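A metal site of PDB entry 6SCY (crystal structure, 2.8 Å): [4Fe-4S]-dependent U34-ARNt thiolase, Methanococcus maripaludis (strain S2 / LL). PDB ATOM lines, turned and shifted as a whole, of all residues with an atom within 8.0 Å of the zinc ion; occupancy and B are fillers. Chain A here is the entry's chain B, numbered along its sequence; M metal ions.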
ATOM      1  N   LYS A   5     -17.973 -22.108  15.694  1.00  0.00           N
ATOM      2  CA  LYS A   5     -17.722 -22.330  17.119  1.00  0.00           C
ATOM      3  C   LYS A   5     -18.963 -22.856  17.860  1.00  0.00           C
ATOM      4  O   LYS A   5     -20.088 -22.546  17.461  1.00  0.00           O
ATOM      5  CB  LYS A   5     -17.128 -21.072  17.795  1.00  0.00           C
ATOM      6  CG  LYS A   5     -17.983 -19.798  17.716  1.00  0.00           C
ATOM      7  CD  LYS A   5     -17.363 -18.645  18.507  1.00  0.00           C
ATOM      8  CE  LYS A   5     -16.149 -18.038  17.843  1.00  0.00           C
ATOM      9  NZ  LYS A   5     -15.539 -16.975  18.682  1.00  0.00           N
ATOM     10  N   CYS A   6     -18.740 -23.691  18.885  1.00  0.00           N
ATOM     11  CA  CYS A   6     -19.773 -24.317  19.707  1.00  0.00           C
ATOM     12  C   CYS A   6     -20.711 -23.292  20.341  1.00  0.00           C
ATOM     13  O   CYS A   6     -20.241 -22.270  20.854  1.00  0.00           O
ATOM     14  CB  CYS A   6     -19.122 -25.201  20.768  1.00  0.00           C
ATOM     15  SG  CYS A   6     -20.291 -26.180  21.730  1.00  0.00           S
ATOM     16  N   ARG A   7     -22.031 -23.554  20.302  1.00  0.00           N
ATOM     17  CA  ARG A   7     -23.062 -22.669  20.857  1.00  0.00           C
ATOM     18  C   ARG A   7     -22.943 -22.490  22.387  1.00  0.00           C
ATOM     19  O   ARG A   7     -23.292 -21.425  22.899  1.00  0.00           O
ATOM     20  CB  ARG A   7     -24.488 -23.135  20.425  1.00  0.00           C
ATOM     21  CG  ARG A   7     -25.452 -23.603  21.536  1.00  0.00           C
ATOM     22  CD  ARG A   7     -26.708 -22.749  21.645  1.00  0.00           C
ATOM     23  NE  ARG A   7     -26.823 -22.113  22.966  1.00  0.00           N
ATOM     24  CZ  ARG A   7     -27.961 -21.934  23.625  1.00  0.00           C
ATOM     25  NH1 ARG A   7     -29.113 -22.352  23.114  1.00  0.00           N
ATOM     26  NH2 ARG A   7     -27.953 -21.356  24.816  1.00  0.00           N
ATOM     27  N   LYS A   8     -22.459 -23.522  23.106  1.00  0.00           N
ATOM     28  CA  LYS A   8     -22.356 -23.521  24.568  1.00  0.00           C
ATOM     29  C   LYS A   8     -20.977 -23.114  25.131  1.00  0.00           C
ATOM     30  O   LYS A   8     -20.941 -22.618  26.260  1.00  0.00           O
ATOM     31  CB  LYS A   8     -22.781 -24.881  25.143  1.00  0.00           C
ATOM     32  CG  LYS A   8     -24.283 -25.156  25.089  1.00  0.00           C
ATOM     33  CD  LYS A   8     -25.043 -24.509  26.254  1.00  0.00           C
ATOM     34  CE  LYS A   8     -26.397 -25.145  26.464  1.00  0.00           C
ATOM     35  NZ  LYS A   8     -27.121 -24.581  27.636  1.00  0.00           N
ATOM     36  N   CYS A   9     -19.866 -23.320  24.389  1.00  0.00           N
ATOM     37  CA  CYS A   9     -18.514 -22.989  24.896  1.00  0.00           C
ATOM     38  C   CYS A   9     -17.596 -22.288  23.890  1.00  0.00           C
ATOM     39  O   CYS A   9     -16.447 -22.017  24.240  1.00  0.00           O
ATOM     40  CB  CYS A   9     -17.842 -24.227  25.481  1.00  0.00           C
ATOM     41  SG  CYS A   9     -17.384 -25.468  24.246  1.00  0.00           S
ATOM     42  N   GLY A  10     -18.079 -22.039  22.663  1.00  0.00           N
ATOM     43  CA  GLY A  10     -17.351 -21.380  21.584  1.00  0.00           C
ATOM     44  C   GLY A  10     -16.124 -22.092  21.048  1.00  0.00           C
ATOM     45  O   GLY A  10     -15.268 -21.463  20.431  1.00  0.00           O
ATOM     46  N   LYS A  11     -16.038 -23.419  21.262  1.00  0.00           N
ATOM     47  CA  LYS A  11     -14.895 -24.226  20.818  1.00  0.00           C
ATOM     48  C   LYS A  11     -15.173 -24.917  19.468  1.00  0.00           C
ATOM     49  O   LYS A  11     -16.355 -25.105  19.153  1.00  0.00           O
ATOM     50  CB  LYS A  11     -14.573 -25.281  21.882  1.00  0.00           C
ATOM     51  CG  LYS A  11     -13.298 -25.029  22.651  1.00  0.00           C
ATOM     52  CD  LYS A  11     -13.060 -26.175  23.615  1.00  0.00           C
ATOM     53  CE  LYS A  11     -13.880 -26.087  24.877  1.00  0.00           C
ATOM     54  NZ  LYS A  11     -14.851 -27.207  24.993  1.00  0.00           N
ATOM     55  N   PRO A  12     -14.143 -25.325  18.672  1.00  0.00           N
ATOM     56  CA  PRO A  12     -14.427 -25.996  17.381  1.00  0.00           C
ATOM     57  C   PRO A  12     -15.449 -27.113  17.546  1.00  0.00           C
ATOM     58  O   PRO A  12     -15.411 -27.869  18.523  1.00  0.00           O
ATOM     59  CB  PRO A  12     -13.065 -26.531  16.957  1.00  0.00           C
ATOM     60  CG  PRO A  12     -12.102 -25.616  17.560  1.00  0.00           C
ATOM     61  CD  PRO A  12     -12.686 -25.189  18.877  1.00  0.00           C
ATOM     62  N   SER A  13     -16.404 -27.178  16.611  1.00  0.00           N
ATOM     63  CA  SER A  13     -17.545 -28.080  16.633  1.00  0.00           C
ATOM     64  C   SER A  13     -17.357 -29.397  15.853  1.00  0.00           C
ATOM     65  O   SER A  13     -16.570 -29.459  14.909  1.00  0.00           O
ATOM     66  CB  SER A  13     -18.785 -27.347  16.160  1.00  0.00           C
ATOM     67  OG  SER A  13     -19.971 -28.117  16.318  1.00  0.00           O
ATOM     68  N   ASN A  23     -24.241 -25.388  16.557  1.00  0.00           N
ATOM     69  CA  ASN A  23     -23.018 -26.180  16.482  1.00  0.00           C
ATOM     70  C   ASN A  23     -22.601 -26.657  17.873  1.00  0.00           C
ATOM     71  O   ASN A  23     -22.639 -25.880  18.826  1.00  0.00           O
ATOM     72  CB  ASN A  23     -21.924 -25.371  15.815  1.00  0.00           C
ATOM     73  CG  ASN A  23     -22.259 -24.910  14.400  1.00  0.00           C
ATOM     74  OD1 ASN A  23     -22.791 -25.659  13.568  1.00  0.00           O
ATOM     75  ND2 ASN A  23     -21.926 -23.659  14.102  1.00  0.00           N
ATOM     76  N   TYR A  24     -22.230 -27.958  17.992  1.00  0.00           N
ATOM     77  CA  TYR A  24     -21.817 -28.563  19.258  1.00  0.00           C
ATOM     78  C   TYR A  24     -20.591 -29.444  19.102  1.00  0.00           C
ATOM     79  O   TYR A  24     -20.538 -30.284  18.202  1.00  0.00           O
ATOM     80  CB  TYR A  24     -22.958 -29.407  19.865  1.00  0.00           C
ATOM     81  CG  TYR A  24     -24.229 -28.646  20.158  1.00  0.00           C
ATOM     82  CD1 TYR A  24     -24.316 -27.776  21.233  1.00  0.00           C
ATOM     83  CD2 TYR A  24     -25.372 -28.859  19.389  1.00  0.00           C
ATOM     84  CE1 TYR A  24     -25.495 -27.083  21.514  1.00  0.00           C
ATOM     85  CE2 TYR A  24     -26.567 -28.175  19.657  1.00  0.00           C
ATOM     86  CZ  TYR A  24     -26.617 -27.278  20.722  1.00  0.00           C
ATOM     87  OH  TYR A  24     -27.785 -26.596  20.986  1.00  0.00           O
ATOM     88  N   CYS A  25     -19.630 -29.298  20.024  1.00  0.00           N
ATOM     89  CA  CYS A  25     -18.430 -30.120  20.086  1.00  0.00           C
ATOM     90  C   CYS A  25     -18.830 -31.443  20.731  1.00  0.00           C
ATOM     91  O   CYS A  25     -19.992 -31.616  21.069  1.00  0.00           O
ATOM     92  CB  CYS A  25     -17.342 -29.410  20.876  1.00  0.00           C
ATOM     93  SG  CYS A  25     -17.787 -29.074  22.602  1.00  0.00           S
ATOM     94  N   LYS A  26     -17.868 -32.366  20.917  1.00  0.00           N
ATOM     95  CA  LYS A  26     -18.140 -33.670  21.534  1.00  0.00           C
ATOM     96  C   LYS A  26     -18.837 -33.545  22.904  1.00  0.00           C
ATOM     97  O   LYS A  26     -19.961 -34.019  23.057  1.00  0.00           O
ATOM     98  CB  LYS A  26     -16.853 -34.511  21.628  1.00  0.00           C
ATOM     99  CG  LYS A  26     -17.072 -35.956  22.064  1.00  0.00           C
ATOM    100  CD  LYS A  26     -15.752 -36.672  22.294  1.00  0.00           C
ATOM    101  CE  LYS A  26     -15.987 -38.048  22.855  1.00  0.00           C
ATOM    102  NZ  LYS A  26     -14.709 -38.770  23.089  1.00  0.00           N
ATOM    103  N   GLU A  27     -18.203 -32.828  23.844  1.00  0.00           N
ATOM    104  CA  GLU A  27     -18.642 -32.625  25.223  1.00  0.00           C
ATOM    105  C   GLU A  27     -19.987 -31.925  25.359  1.00  0.00           C
ATOM    106  O   GLU A  27     -20.789 -32.322  26.212  1.00  0.00           O
ATOM    107  CB  GLU A  27     -17.573 -31.894  26.023  1.00  0.00           C
ATOM    108  CG  GLU A  27     -16.219 -32.589  26.086  1.00  0.00           C
ATOM    109  CD  GLU A  27     -15.347 -32.592  24.836  1.00  0.00           C
ATOM    110  OE1 GLU A  27     -15.347 -31.603  24.083  1.00  0.00           O
ATOM    111  OE2 GLU A  27     -14.679 -33.632  24.602  1.00  0.00           O
ATOM    112  N   CYS A  28     -20.241 -30.901  24.542  1.00  0.00           N
ATOM    113  CA  CYS A  28     -21.495 -30.146  24.556  1.00  0.00           C
ATOM    114  C   CYS A  28     -22.650 -30.872  23.879  1.00  0.00           C
ATOM    115  O   CYS A  28     -23.803 -30.614  24.215  1.00  0.00           O
ATOM    116  CB  CYS A  28     -21.309 -28.745  23.979  1.00  0.00           C
ATOM    117  SG  CYS A  28     -20.282 -27.663  25.008  1.00  0.00           S
ATOM    118  N   PHE A  29     -22.347 -31.783  22.914  1.00  0.00           N
ATOM    119  CA  PHE A  29     -23.342 -32.593  22.203  1.00  0.00           C
ATOM    120  C   PHE A  29     -23.888 -33.688  23.142  1.00  0.00           C
ATOM    121  O   PHE A  29     -25.103 -33.921  23.185  1.00  0.00           O
ATOM    122  CB  PHE A  29     -22.771 -33.201  20.911  1.00  0.00           C
ATOM    123  CG  PHE A  29     -23.725 -34.156  20.227  1.00  0.00           C
ATOM    124  CD1 PHE A  29     -24.884 -33.698  19.615  1.00  0.00           C
ATOM    125  CD2 PHE A  29     -23.480 -35.524  20.236  1.00  0.00           C
ATOM    126  CE1 PHE A  29     -25.779 -34.589  19.026  1.00  0.00           C
ATOM    127  CE2 PHE A  29     -24.383 -36.415  19.641  1.00  0.00           C
ATOM    128  CZ  PHE A  29     -25.525 -35.948  19.042  1.00  0.00           C
ATOM    129  N   LYS A  31     -23.839 -33.589  26.435  1.00  0.00           N
ATOM    130  CA  LYS A  31     -24.518 -32.846  27.494  1.00  0.00           C
ATOM    131  C   LYS A  31     -25.921 -32.410  27.073  1.00  0.00           C
ATOM    132  O   LYS A  31     -26.826 -32.426  27.913  1.00  0.00           O
ATOM    133  CB  LYS A  31     -23.674 -31.635  27.885  1.00  0.00           C
ATOM    134  CG  LYS A  31     -23.772 -31.234  29.346  1.00  0.00           C
ATOM    135  CD  LYS A  31     -22.988 -29.943  29.597  1.00  0.00           C
ATOM    136  CE  LYS A  31     -21.491 -30.113  29.823  1.00  0.00           C
ATOM    137  NZ  LYS A  31     -20.751 -28.868  29.530  1.00  0.00           N
HETATM  138 ZN    ZN M   1     -18.856 -26.968  23.511  1.00  0.00          ZN
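The side-chain amino group (NZ) of Lys 11 lies close to the side-chain sulfur (SG) of Cys 9, 3.2 Å away. The backbone NH (N) of Cys 6 sits at hydrogen-bond distance from the backbone carbonyl oxygen (O) of Lys 11 (2.8 Å). The backbone NH of Lys 8 sits close to the side-chain sulfur of Cys 6. The backbone carbonyl oxygen (O) of Asn 23 sits close to the side-chain sulfur (SG) of Cys 6 (3.7 Å).
Within 4 Å of the zinc ion: Cys 6, Cys 9, Cys 25 and Cys 28. The nearest printed residue that does not touch the zinc ion is Lys 11 (4.3 Å).
The zinc ion is bound by SG of Cys 28 (2.2 Å), SG of Cys 9 (2.2 Å), SG of Cys 6 (2.4 Å) and SG of Cys 25 (2.5 Å).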
